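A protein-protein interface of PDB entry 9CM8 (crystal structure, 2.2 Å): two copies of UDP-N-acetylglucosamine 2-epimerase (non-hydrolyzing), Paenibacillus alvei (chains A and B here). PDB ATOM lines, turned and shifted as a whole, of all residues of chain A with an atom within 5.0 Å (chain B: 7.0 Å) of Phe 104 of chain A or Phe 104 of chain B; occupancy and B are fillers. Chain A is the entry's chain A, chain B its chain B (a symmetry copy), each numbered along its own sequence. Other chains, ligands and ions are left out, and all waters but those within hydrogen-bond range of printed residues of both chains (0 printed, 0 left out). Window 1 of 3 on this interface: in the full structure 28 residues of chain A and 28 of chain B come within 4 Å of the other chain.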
ATOM      1  N   THR A 100     -14.106 -14.127  -0.425  1.00  0.00           N
ATOM      2  CA  THR A 100     -15.068 -13.054  -0.067  1.00  0.00           C
ATOM      3  C   THR A 100     -14.806 -12.631   1.373  1.00  0.00           C
ATOM      4  O   THR A 100     -14.169 -13.393   2.109  1.00  0.00           O
ATOM      5  CB  THR A 100     -16.525 -13.519  -0.197  1.00  0.00           C
ATOM      6  OG1 THR A 100     -16.689 -14.638   0.673  1.00  0.00           O
ATOM      7  CG2 THR A 100     -16.905 -13.919  -1.603  1.00  0.00           C
ATOM      8  N   LEU A 101     -15.355 -11.490   1.790  1.00  0.00           N
ATOM      9  CA  LEU A 101     -15.303 -11.049   3.214  1.00  0.00           C
ATOM     10  C   LEU A 101     -16.008 -12.098   4.098  1.00  0.00           C
ATOM     11  O   LEU A 101     -15.503 -12.423   5.185  1.00  0.00           O
ATOM     12  CB  LEU A 101     -15.941  -9.656   3.284  1.00  0.00           C
ATOM     13  CG  LEU A 101     -15.611  -8.816   4.520  1.00  0.00           C
ATOM     14  CD1 LEU A 101     -14.126  -8.481   4.608  1.00  0.00           C
ATOM     15  CD2 LEU A 101     -16.446  -7.547   4.518  1.00  0.00           C
ATOM     16  N   THR A 102     -17.080 -12.703   3.603  1.00  0.00           N
ATOM     17  CA  THR A 102     -17.893 -13.728   4.312  1.00  0.00           C
ATOM     18  C   THR A 102     -17.056 -14.968   4.613  1.00  0.00           C
ATOM     19  O   THR A 102     -17.235 -15.550   5.677  1.00  0.00           O
ATOM     20  CB  THR A 102     -19.129 -14.088   3.474  1.00  0.00           C
ATOM     21  OG1 THR A 102     -19.985 -12.954   3.593  1.00  0.00           O
ATOM     22  CG2 THR A 102     -19.859 -15.320   3.955  1.00  0.00           C
ATOM     23  N   THR A 103     -16.190 -15.370   3.686  1.00  0.00           N
ATOM     24  CA  THR A 103     -15.313 -16.555   3.825  1.00  0.00           C
ATOM     25  C   THR A 103     -14.465 -16.356   5.065  1.00  0.00           C
ATOM     26  O   THR A 103     -14.437 -17.241   5.934  1.00  0.00           O
ATOM     27  CB  THR A 103     -14.409 -16.719   2.612  1.00  0.00           C
ATOM     28  OG1 THR A 103     -15.354 -16.813   1.547  1.00  0.00           O
ATOM     29  CG2 THR A 103     -13.468 -17.900   2.716  1.00  0.00           C
ATOM     30  N   PHE A 104     -13.814 -15.202   5.151  1.00  0.00           N
ATOM     31  CA  PHE A 104     -12.963 -14.900   6.312  1.00  0.00           C
ATOM     32  C   PHE A 104     -13.825 -14.774   7.576  1.00  0.00           C
ATOM     33  O   PHE A 104     -13.486 -15.405   8.568  1.00  0.00           O
ATOM     34  CB  PHE A 104     -12.140 -13.644   6.060  1.00  0.00           C
ATOM     35  CG  PHE A 104     -11.629 -13.111   7.359  1.00  0.00           C
ATOM     36  CD1 PHE A 104     -10.769 -13.874   8.122  1.00  0.00           C
ATOM     37  CD2 PHE A 104     -12.094 -11.904   7.853  1.00  0.00           C
ATOM     38  CE1 PHE A 104     -10.340 -13.412   9.351  1.00  0.00           C
ATOM     39  CE2 PHE A 104     -11.641 -11.445   9.072  1.00  0.00           C
ATOM     40  CZ  PHE A 104     -10.766 -12.198   9.804  1.00  0.00           C
ATOM     41  N   LEU A 105     -14.870 -13.946   7.563  1.00  0.00           N
ATOM     42  CA  LEU A 105     -15.710 -13.657   8.765  1.00  0.00           C
ATOM     43  C   LEU A 105     -16.306 -14.964   9.308  1.00  0.00           C
ATOM     44  O   LEU A 105     -16.262 -15.182  10.547  1.00  0.00           O
ATOM     45  CB  LEU A 105     -16.835 -12.687   8.391  1.00  0.00           C
ATOM     46  CG  LEU A 105     -16.582 -11.181   8.558  1.00  0.00           C
ATOM     47  CD1 LEU A 105     -15.551 -10.853   9.614  1.00  0.00           C
ATOM     48  CD2 LEU A 105     -16.211 -10.544   7.257  1.00  0.00           C
ATOM     49  N   ALA A 106     -16.839 -15.822   8.434  1.00  0.00           N
ATOM     50  CA  ALA A 106     -17.424 -17.111   8.871  1.00  0.00           C
ATOM     51  C   ALA A 106     -16.336 -17.984   9.500  1.00  0.00           C
ATOM     52  O   ALA A 106     -16.655 -18.675  10.493  1.00  0.00           O
ATOM     53  CB  ALA A 106     -18.134 -17.794   7.736  1.00  0.00           C
ATOM     54  N   SER A 107     -15.099 -17.981   8.960  1.00  0.00           N
ATOM     55  CA  SER A 107     -13.988 -18.816   9.491  1.00  0.00           C
ATOM     56  C   SER A 107     -13.684 -18.320  10.899  1.00  0.00           C
ATOM     57  O   SER A 107     -13.442 -19.136  11.789  1.00  0.00           O
ATOM     58  CB  SER A 107     -12.735 -18.759   8.663  1.00  0.00           C
ATOM     59  OG  SER A 107     -12.962 -19.112   7.319  1.00  0.00           O
ATOM     60  N   TYR A 108     -13.686 -17.001  11.057  1.00  0.00           N
ATOM     61  CA  TYR A 108     -13.372 -16.283  12.322  1.00  0.00           C
ATOM     62  C   TYR A 108     -14.482 -16.530  13.363  1.00  0.00           C
ATOM     63  O   TYR A 108     -14.187 -16.862  14.533  1.00  0.00           O
ATOM     64  CB  TYR A 108     -13.115 -14.811  11.992  1.00  0.00           C
ATOM     65  CG  TYR A 108     -12.728 -14.028  13.209  1.00  0.00           C
ATOM     66  CD1 TYR A 108     -11.526 -14.266  13.845  1.00  0.00           C
ATOM     67  CD2 TYR A 108     -13.617 -13.138  13.784  1.00  0.00           C
ATOM     68  CE1 TYR A 108     -11.193 -13.597  15.011  1.00  0.00           C
ATOM     69  CE2 TYR A 108     -13.299 -12.458  14.946  1.00  0.00           C
ATOM     70  CZ  TYR A 108     -12.084 -12.688  15.558  1.00  0.00           C
ATOM     71  OH  TYR A 108     -11.804 -12.027  16.705  1.00  0.00           O
ATOM     72  N   ASN A 138      -8.315 -11.386   2.401  1.00  0.00           N
ATOM     73  CA  ASN A 138      -9.401 -12.297   2.828  1.00  0.00           C
ATOM     74  C   ASN A 138      -8.920 -13.744   2.761  1.00  0.00           C
ATOM     75  O   ASN A 138      -9.149 -14.441   3.737  1.00  0.00           O
ATOM     76  CB  ASN A 138     -10.668 -12.121   1.992  1.00  0.00           C
ATOM     77  CG  ASN A 138     -11.403 -10.843   2.336  1.00  0.00           C
ATOM     78  OD1 ASN A 138     -11.220 -10.305   3.432  1.00  0.00           O
ATOM     79  ND2 ASN A 138     -12.217 -10.365   1.393  1.00  0.00           N
ATOM     80  N   LEU A 141      -6.068 -14.517   5.382  1.00  0.00           N
ATOM     81  CA  LEU A 141      -6.665 -14.621   6.742  1.00  0.00           C
ATOM     82  C   LEU A 141      -7.362 -15.974   6.888  1.00  0.00           C
ATOM     83  O   LEU A 141      -7.161 -16.615   7.904  1.00  0.00           O
ATOM     84  CB  LEU A 141      -7.631 -13.460   6.991  1.00  0.00           C
ATOM     85  CG  LEU A 141      -6.976 -12.082   7.019  1.00  0.00           C
ATOM     86  CD1 LEU A 141      -8.011 -10.982   6.852  1.00  0.00           C
ATOM     87  CD2 LEU A 141      -6.191 -11.877   8.315  1.00  0.00           C
ATOM     88  N   THR A 142      -8.163 -16.390   5.909  1.00  0.00           N
ATOM     89  CA  THR A 142      -8.877 -17.692   5.926  1.00  0.00           C
ATOM     90  C   THR A 142      -7.805 -18.789   6.028  1.00  0.00           C
ATOM     91  O   THR A 142      -7.952 -19.747   6.839  1.00  0.00           O
ATOM     92  CB  THR A 142      -9.815 -17.785   4.709  1.00  0.00           C
ATOM     93  OG1 THR A 142     -10.757 -16.721   4.782  1.00  0.00           O
ATOM     94  CG2 THR A 142     -10.576 -19.084   4.609  1.00  0.00           C
ATOM     95  N   LEU A 145      -6.870 -19.459   9.453  1.00  0.00           N
ATOM     96  CA  LEU A 145      -7.957 -20.004  10.308  1.00  0.00           C
ATOM     97  C   LEU A 145      -8.312 -21.449   9.906  1.00  0.00           C
ATOM     98  O   LEU A 145      -8.784 -22.223  10.786  1.00  0.00           O
ATOM     99  CB  LEU A 145      -9.160 -19.052  10.226  1.00  0.00           C
ATOM    100  CG  LEU A 145      -9.053 -17.751  11.023  1.00  0.00           C
ATOM    101  CD1 LEU A 145     -10.217 -16.827  10.713  1.00  0.00           C
ATOM    102  CD2 LEU A 145      -9.047 -18.022  12.505  1.00  0.00           C
ATOM    103  N   SER B  75     -14.830  -8.847  19.988  1.00  0.00           N
ATOM    104  CA  SER B  75     -14.538  -8.671  18.553  1.00  0.00           C
ATOM    105  C   SER B  75     -15.469  -7.608  17.994  1.00  0.00           C
ATOM    106  O   SER B  75     -14.947  -6.604  17.460  1.00  0.00           O
ATOM    107  CB  SER B  75     -14.609  -9.969  17.807  1.00  0.00           C
ATOM    108  OG  SER B  75     -13.608 -10.850  18.297  1.00  0.00           O
ATOM    109  N   LEU B  79     -14.260  -3.498  17.062  1.00  0.00           N
ATOM    110  CA  LEU B  79     -14.465  -3.059  15.653  1.00  0.00           C
ATOM    111  C   LEU B  79     -15.383  -1.825  15.609  1.00  0.00           C
ATOM    112  O   LEU B  79     -14.998  -0.828  14.963  1.00  0.00           O
ATOM    113  CB  LEU B  79     -15.051  -4.213  14.846  1.00  0.00           C
ATOM    114  CG  LEU B  79     -14.094  -4.965  13.923  1.00  0.00           C
ATOM    115  CD1 LEU B  79     -12.637  -4.822  14.331  1.00  0.00           C
ATOM    116  CD2 LEU B  79     -14.482  -6.428  13.845  1.00  0.00           C
ATOM    117  N   VAL B  96       0.429  -2.004  17.027  1.00  0.00           N
ATOM    118  CA  VAL B  96      -0.228  -3.025  17.888  1.00  0.00           C
ATOM    119  C   VAL B  96       0.859  -3.963  18.442  1.00  0.00           C
ATOM    120  O   VAL B  96       1.966  -4.079  17.842  1.00  0.00           O
ATOM    121  CB  VAL B  96      -1.281  -3.768  17.048  1.00  0.00           C
ATOM    122  CG1 VAL B  96      -2.378  -2.817  16.602  1.00  0.00           C
ATOM    123  CG2 VAL B  96      -0.671  -4.455  15.830  1.00  0.00           C
ATOM    124  N   HIS B  97       0.572  -4.613  19.556  1.00  0.00           N
ATOM    125  CA  HIS B  97       1.591  -5.348  20.326  1.00  0.00           C
ATOM    126  C   HIS B  97       1.166  -6.795  20.554  1.00  0.00           C
ATOM    127  O   HIS B  97       0.015  -7.034  20.874  1.00  0.00           O
ATOM    128  CB  HIS B  97       1.878  -4.648  21.647  1.00  0.00           C
ATOM    129  CG  HIS B  97       2.991  -5.328  22.346  1.00  0.00           C
ATOM    130  ND1 HIS B  97       2.799  -6.493  23.026  1.00  0.00           N
ATOM    131  CD2 HIS B  97       4.302  -5.067  22.387  1.00  0.00           C
ATOM    132  CE1 HIS B  97       3.942  -6.891  23.517  1.00  0.00           C
ATOM    133  NE2 HIS B  97       4.869  -6.035  23.152  1.00  0.00           N
ATOM    134  N   GLY B  98       2.080  -7.722  20.339  1.00  0.00           N
ATOM    135  CA  GLY B  98       1.958  -9.110  20.825  1.00  0.00           C
ATOM    136  C   GLY B  98       0.813  -9.869  20.192  1.00  0.00           C
ATOM    137  O   GLY B  98       0.602  -9.765  18.975  1.00  0.00           O
ATOM    138  N   ASP B  99       0.117 -10.647  21.006  1.00  0.00           N
ATOM    139  CA  ASP B  99      -0.723 -11.757  20.514  1.00  0.00           C
ATOM    140  C   ASP B  99      -2.067 -11.744  21.230  1.00  0.00           C
ATOM    141  O   ASP B  99      -2.695 -12.814  21.358  1.00  0.00           O
ATOM    142  CB  ASP B  99       0.028 -13.073  20.643  1.00  0.00           C
ATOM    143  CG  ASP B  99       0.915 -13.153  21.852  1.00  0.00           C
ATOM    144  OD1 ASP B  99       0.376 -12.932  22.968  1.00  0.00           O
ATOM    145  OD2 ASP B  99       2.141 -13.414  21.644  1.00  0.00           O
ATOM    146  N   THR B 100      -2.512 -10.553  21.611  1.00  0.00           N
ATOM    147  CA  THR B 100      -3.858 -10.330  22.192  1.00  0.00           C
ATOM    148  C   THR B 100      -4.909 -10.307  21.066  1.00  0.00           C
ATOM    149  O   THR B 100      -4.576 -10.076  19.897  1.00  0.00           O
ATOM    150  CB  THR B 100      -3.777  -9.082  23.073  1.00  0.00           C
ATOM    151  OG1 THR B 100      -4.818  -9.182  24.037  1.00  0.00           O
ATOM    152  CG2 THR B 100      -3.932  -7.817  22.283  1.00  0.00           C
ATOM    153  N   LEU B 101      -6.186 -10.521  21.383  1.00  0.00           N
ATOM    154  CA  LEU B 101      -7.288 -10.495  20.377  1.00  0.00           C
ATOM    155  C   LEU B 101      -7.382  -9.077  19.819  1.00  0.00           C
ATOM    156  O   LEU B 101      -7.656  -8.880  18.601  1.00  0.00           O
ATOM    157  CB  LEU B 101      -8.601 -10.885  21.067  1.00  0.00           C
ATOM    158  CG  LEU B 101      -9.482 -11.916  20.365  1.00  0.00           C
ATOM    159  CD1 LEU B 101     -10.939 -11.689  20.740  1.00  0.00           C
ATOM    160  CD2 LEU B 101      -9.325 -11.900  18.852  1.00  0.00           C
ATOM    161  N   THR B 102      -7.164  -8.111  20.703  1.00  0.00           N
ATOM    162  CA  THR B 102      -7.279  -6.652  20.436  1.00  0.00           C
ATOM    163  C   THR B 102      -6.223  -6.200  19.407  1.00  0.00           C
ATOM    164  O   THR B 102      -6.547  -5.380  18.524  1.00  0.00           O
ATOM    165  CB  THR B 102      -7.165  -5.907  21.771  1.00  0.00           C
ATOM    166  OG1 THR B 102      -8.424  -6.129  22.402  1.00  0.00           O
ATOM    167  CG2 THR B 102      -6.910  -4.431  21.615  1.00  0.00           C
ATOM    168  N   THR B 103      -5.016  -6.743  19.501  1.00  0.00           N
ATOM    169  CA  THR B 103      -3.919  -6.539  18.521  1.00  0.00           C
ATOM    170  C   THR B 103      -4.429  -6.935  17.135  1.00  0.00           C
ATOM    171  O   THR B 103      -4.306  -6.132  16.196  1.00  0.00           O
ATOM    172  CB  THR B 103      -2.676  -7.285  19.013  1.00  0.00           C
ATOM    173  OG1 THR B 103      -2.302  -6.448  20.105  1.00  0.00           O
ATOM    174  CG2 THR B 103      -1.578  -7.435  17.991  1.00  0.00           C
ATOM    175  N   PHE B 104      -5.067  -8.097  17.028  1.00  0.00           N
ATOM    176  CA  PHE B 104      -5.602  -8.547  15.727  1.00  0.00           C
ATOM    177  C   PHE B 104      -6.741  -7.602  15.308  1.00  0.00           C
ATOM    178  O   PHE B 104      -6.765  -7.121  14.155  1.00  0.00           O
ATOM    179  CB  PHE B 104      -6.023 -10.014  15.775  1.00  0.00           C
ATOM    180  CG  PHE B 104      -7.010 -10.311  14.686  1.00  0.00           C
ATOM    181  CD1 PHE B 104      -6.658 -10.136  13.367  1.00  0.00           C
ATOM    182  CD2 PHE B 104      -8.309 -10.651  14.988  1.00  0.00           C
ATOM    183  CE1 PHE B 104      -7.580 -10.353  12.356  1.00  0.00           C
ATOM    184  CE2 PHE B 104      -9.230 -10.868  13.978  1.00  0.00           C
ATOM    185  CZ  PHE B 104      -8.858 -10.734  12.668  1.00  0.00           C
ATOM    186  N   LEU B 105      -7.697  -7.358  16.200  1.00  0.00           N
ATOM    187  CA  LEU B 105      -8.915  -6.554  15.862  1.00  0.00           C
ATOM    188  C   LEU B 105      -8.492  -5.160  15.370  1.00  0.00           C
ATOM    189  O   LEU B 105      -9.073  -4.681  14.357  1.00  0.00           O
ATOM    190  CB  LEU B 105      -9.824  -6.434  17.094  1.00  0.00           C
ATOM    191  CG  LEU B 105     -10.882  -7.515  17.315  1.00  0.00           C
ATOM    192  CD1 LEU B 105     -11.090  -8.416  16.126  1.00  0.00           C
ATOM    193  CD2 LEU B 105     -10.571  -8.316  18.539  1.00  0.00           C
ATOM    194  N   ALA B 106      -7.561  -4.528  16.090  1.00  0.00           N
ATOM    195  CA  ALA B 106      -7.038  -3.176  15.786  1.00  0.00           C
ATOM    196  C   ALA B 106      -6.370  -3.210  14.414  1.00  0.00           C
ATOM    197  O   ALA B 106      -6.643  -2.311  13.597  1.00  0.00           O
ATOM    198  CB  ALA B 106      -6.096  -2.729  16.880  1.00  0.00           C
ATOM    199  N   SER B 107      -5.581  -4.253  14.142  1.00  0.00           N
ATOM    200  CA  SER B 107      -4.952  -4.482  12.819  1.00  0.00           C
ATOM    201  C   SER B 107      -6.045  -4.620  11.752  1.00  0.00           C
ATOM    202  O   SER B 107      -5.892  -3.994  10.651  1.00  0.00           O
ATOM    203  CB  SER B 107      -4.024  -5.681  12.836  1.00  0.00           C
ATOM    204  OG  SER B 107      -3.115  -5.602  13.941  1.00  0.00           O
ATOM    205  N   TYR B 108      -7.092  -5.408  12.026  1.00  0.00           N
ATOM    206  CA  TYR B 108      -8.236  -5.631  11.089  1.00  0.00           C
ATOM    207  C   TYR B 108      -8.987  -4.301  10.874  1.00  0.00           C
ATOM    208  O   TYR B 108      -9.240  -3.929   9.718  1.00  0.00           O
ATOM    209  CB  TYR B 108      -9.134  -6.778  11.576  1.00  0.00           C
ATOM    210  CG  TYR B 108     -10.259  -7.114  10.634  1.00  0.00           C
ATOM    211  CD1 TYR B 108      -9.992  -7.613   9.379  1.00  0.00           C
ATOM    212  CD2 TYR B 108     -11.581  -6.889  10.969  1.00  0.00           C
ATOM    213  CE1 TYR B 108     -11.004  -7.885   8.478  1.00  0.00           C
ATOM    214  CE2 TYR B 108     -12.617  -7.161  10.092  1.00  0.00           C
ATOM    215  CZ  TYR B 108     -12.324  -7.651   8.834  1.00  0.00           C
ATOM    216  OH  TYR B 108     -13.306  -7.912   7.928  1.00  0.00           O
ATOM    217  N   ALA B 109      -9.283  -3.555  11.943  1.00  0.00           N
ATOM    218  CA  ALA B 109      -9.961  -2.236  11.852  1.00  0.00           C
ATOM    219  C   ALA B 109      -9.146  -1.309  10.936  1.00  0.00           C
ATOM    220  O   ALA B 109      -9.730  -0.654  10.026  1.00  0.00           O
ATOM    221  CB  ALA B 109     -10.139  -1.657  13.237  1.00  0.00           C
ATOM    222  N   ALA B 110      -7.828  -1.271  11.139  1.00  0.00           N
ATOM    223  CA  ALA B 110      -6.875  -0.465  10.339  1.00  0.00           C
ATOM    224  C   ALA B 110      -6.910  -0.913   8.876  1.00  0.00           C
ATOM    225  O   ALA B 110      -6.975  -0.060   7.989  1.00  0.00           O
ATOM    226  CB  ALA B 110      -5.491  -0.604  10.926  1.00  0.00           C
ATOM    227  N   MET B 137      -2.962 -18.214  17.062  1.00  0.00           N
ATOM    228  CA  MET B 137      -3.849 -17.833  15.949  1.00  0.00           C
ATOM    229  C   MET B 137      -3.917 -16.304  15.864  1.00  0.00           C
ATOM    230  O   MET B 137      -3.802 -15.776  14.754  1.00  0.00           O
ATOM    231  CB  MET B 137      -5.254 -18.418  16.151  1.00  0.00           C
ATOM    232  CG  MET B 137      -6.071 -18.409  14.885  1.00  0.00           C
ATOM    233  SD  MET B 137      -5.648 -19.695  13.640  1.00  0.00           S
ATOM    234  CE  MET B 137      -4.214 -20.542  14.314  1.00  0.00           C
ATOM    235  N   ASN B 138      -4.052 -15.613  16.990  1.00  0.00           N
ATOM    236  CA  ASN B 138      -4.097 -14.125  17.022  1.00  0.00           C
ATOM    237  C   ASN B 138      -2.827 -13.547  16.379  1.00  0.00           C
ATOM    238  O   ASN B 138      -2.971 -12.676  15.536  1.00  0.00           O
ATOM    239  CB  ASN B 138      -4.246 -13.554  18.432  1.00  0.00           C
ATOM    240  CG  ASN B 138      -5.611 -13.770  19.058  1.00  0.00           C
ATOM    241  OD1 ASN B 138      -6.593 -13.977  18.353  1.00  0.00           O
ATOM    242  ND2 ASN B 138      -5.678 -13.683  20.380  1.00  0.00           N
ATOM    243  N   ARG B 139      -1.631 -13.986  16.782  1.00  0.00           N
ATOM    244  CA  ARG B 139      -0.358 -13.438  16.222  1.00  0.00           C
ATOM    245  C   ARG B 139      -0.145 -13.838  14.765  1.00  0.00           C
ATOM    246  O   ARG B 139       0.530 -13.047  14.043  1.00  0.00           O
ATOM    247  CB  ARG B 139       0.873 -13.762  17.075  1.00  0.00           C
ATOM    248  CG  ARG B 139       1.196 -15.224  17.294  1.00  0.00           C
ATOM    249  CD  ARG B 139       1.878 -15.375  18.653  1.00  0.00           C
ATOM    250  NE  ARG B 139       2.249 -16.759  18.913  1.00  0.00           N
ATOM    251  CZ  ARG B 139       2.563 -17.267  20.110  1.00  0.00           C
ATOM    252  NH1 ARG B 139       2.585 -16.512  21.186  1.00  0.00           N
ATOM    253  NH2 ARG B 139       2.852 -18.546  20.227  1.00  0.00           N
ATOM    254  N   GLN B 140      -0.685 -14.974  14.318  1.00  0.00           N
ATOM    255  CA  GLN B 140      -0.629 -15.342  12.883  1.00  0.00           C
ATOM    256  C   GLN B 140      -1.570 -14.419  12.102  1.00  0.00           C
ATOM    257  O   GLN B 140      -1.158 -13.959  11.022  1.00  0.00           O
ATOM    258  CB  GLN B 140      -0.924 -16.824  12.660  1.00  0.00           C
ATOM    259  CG  GLN B 140       0.160 -17.753  13.209  1.00  0.00           C
ATOM    260  CD  GLN B 140      -0.141 -19.185  12.844  1.00  0.00           C
ATOM    261  OE1 GLN B 140      -0.714 -19.448  11.797  1.00  0.00           O
ATOM    262  NE2 GLN B 140       0.224 -20.116  13.712  1.00  0.00           N
ATOM    263  N   LEU B 141      -2.792 -14.178  12.611  1.00  0.00           N
ATOM    264  CA  LEU B 141      -3.774 -13.275  11.950  1.00  0.00           C
ATOM    265  C   LEU B 141      -3.154 -11.883  11.851  1.00  0.00           C
ATOM    266  O   LEU B 141      -3.202 -11.331  10.745  1.00  0.00           O
ATOM    267  CB  LEU B 141      -5.115 -13.221  12.704  1.00  0.00           C
ATOM    268  CG  LEU B 141      -5.982 -14.481  12.612  1.00  0.00           C
ATOM    269  CD1 LEU B 141      -7.148 -14.403  13.595  1.00  0.00           C
ATOM    270  CD2 LEU B 141      -6.510 -14.666  11.206  1.00  0.00           C
ATOM    271  N   THR B 142      -2.651 -11.327  12.959  1.00  0.00           N
ATOM    272  CA  THR B 142      -1.921 -10.017  12.960  1.00  0.00           C
ATOM    273  C   THR B 142      -0.798 -10.062  11.907  1.00  0.00           C
ATOM    274  O   THR B 142      -0.673  -9.126  11.066  1.00  0.00           O
ATOM    275  CB  THR B 142      -1.430  -9.658  14.374  1.00  0.00           C
ATOM    276  OG1 THR B 142      -2.598  -9.685  15.183  1.00  0.00           O
ATOM    277  CG2 THR B 142      -0.771  -8.298  14.476  1.00  0.00           C
ATOM    278  N   GLY B 143      -0.035 -11.138  11.903  1.00  0.00           N
ATOM    279  CA  GLY B 143       1.037 -11.382  10.919  1.00  0.00           C
ATOM    280  C   GLY B 143       0.580 -11.186   9.486  1.00  0.00           C
ATOM    281  O   GLY B 143       1.384 -10.630   8.675  1.00  0.00           O
ATOM    282  N   VAL B 144      -0.634 -11.585   9.117  1.00  0.00           N
ATOM    283  CA  VAL B 144      -1.026 -11.363   7.694  1.00  0.00           C
ATOM    284  C   VAL B 144      -1.477  -9.900   7.492  1.00  0.00           C
ATOM    285  O   VAL B 144      -1.316  -9.408   6.385  1.00  0.00           O
ATOM    286  CB  VAL B 144      -2.023 -12.381   7.095  1.00  0.00           C
ATOM    287  CG1 VAL B 144      -1.825 -13.812   7.556  1.00  0.00           C
ATOM    288  CG2 VAL B 144      -3.450 -11.964   7.247  1.00  0.00           C
ATOM    289  N   LEU B 145      -1.966  -9.191   8.505  1.00  0.00           N
ATOM    290  CA  LEU B 145      -2.404  -7.772   8.322  1.00  0.00           C
ATOM    291  C   LEU B 145      -1.238  -6.767   8.447  1.00  0.00           C
ATOM    292  O   LEU B 145      -1.347  -5.666   7.917  1.00  0.00           O
ATOM    293  CB  LEU B 145      -3.485  -7.454   9.354  1.00  0.00           C
ATOM    294  CG  LEU B 145      -4.857  -8.117   9.151  1.00  0.00           C
ATOM    295  CD1 LEU B 145      -5.229  -8.963  10.345  1.00  0.00           C
ATOM    296  CD2 LEU B 145      -5.933  -7.082   9.018  1.00  0.00           C
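The side-chain hydroxyl of Ser 75 of chain B is in hydrogen-bond range of the side-chain hydroxyl of Tyr 108 of chain A, at 2.7 Å.
ND2 of Asn 138 of chain A lies close to N of Leu 101 of chain A, at 3.4 Å. The backbone NH (N) of Phe 104 of chain A lies close to the side-chain hydroxyl (OG1) of Thr 142 of chain A (3.4 Å). The side-chain amide nitrogen (ND2) of Asn 138 of chain B lies close to the backbone NH (N) of Leu 101 of chain B (3.4 Å). The backbone NH of Phe 104 of chain B sits close to the side-chain hydroxyl of Thr 142 of chain B, at 3.5 Å.
Tyr 108 of chain B touches Leu 101 of chain A. Phe 104 of chain B touches Phe 104 of chain A. CE2 of Phe 104 of chain A touches CE1 of Tyr 108 of chain B (3.7 Å). Leu 105 of chain A touches Tyr 108 of chain B (CD2 to OH, 3.98 Å). Tyr 108 of chain A touches Leu 101 of chain B (OH to CD2, 3.3 Å). CE1 of Tyr 108 of chain A touches CE2 of Phe 104 of chain B, at 3.5 Å. CD1 of Leu 105 of chain B touches OH of Tyr 108 of chain A (3.7 Å). Leu 141 of chain A touches Leu 141 of chain B. CD2 of Leu 141 of chain A touches CG2 of Val 144 of chain B, at 2.9 Å. Met 137 of chain B touches Leu 145 of chain A.
Of the printed residues of chain B, Leu 101 of chain A touches Tyr 108. Phe 104 of chain A touches just these residues of chain B: Phe 104 (3.7 Å) and Tyr 108 (3.7 Å). Of the printed residues of chain B, Tyr 108 of chain A touches Ser 75 (2.7 Å), Leu 101 (3.3 Å), Phe 104 (3.5 Å) and Leu 105 (3.7 Å). Gly 98 of chain B touches none of the printed residues of chain A. Of the printed residues of chain A, Leu 105 of chain B touches Tyr 108. Of the printed residues of chain A, Val 144 of chain B touches Leu 141 (2.9 Å). The nearest residue of chain B that does not touch Phe 104 of chain A is Leu 141 of chain B (4.4 Å). The nearest printed residue of chain A that does not touch Ser 75 of chain B is Leu 105 of chain A (8.3 Å).
Of the 13 printed residues of chain A, 6 touch a printed residue of chain B. Printed residues of chain A that touch a printed residue of chain B: Leu 101, Phe 104, Leu 105, Tyr 108, Leu 141 and Leu 145. Of the 26 printed residues of chain B, 9 touch a printed residue of chain A. Hydrophobic or aromatic side chains of chain B within 4 Å of the printed part of chain A: Leu 101, Phe 104, Leu 105, Tyr 108, Met 137, Leu 141, Val 144 and Leu 145.
Leu 101 of chain A touches Tyr 108 of chain B, and with the chains exchanged Tyr 108 of chain A touches Leu 101 of chain B. Phe 104 of chain A touches its own counterpart, Phe 104 of chain B. Phe 104 of chain A touches Tyr 108 of chain B, and with the chains exchanged Tyr 108 of chain A touches Phe 104 of chain B. Leu 105 of chain A touches Tyr 108 of chain B, and with the chains exchanged Tyr 108 of chain A touches Leu 105 of chain B. 13 positions are printed for both chains.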
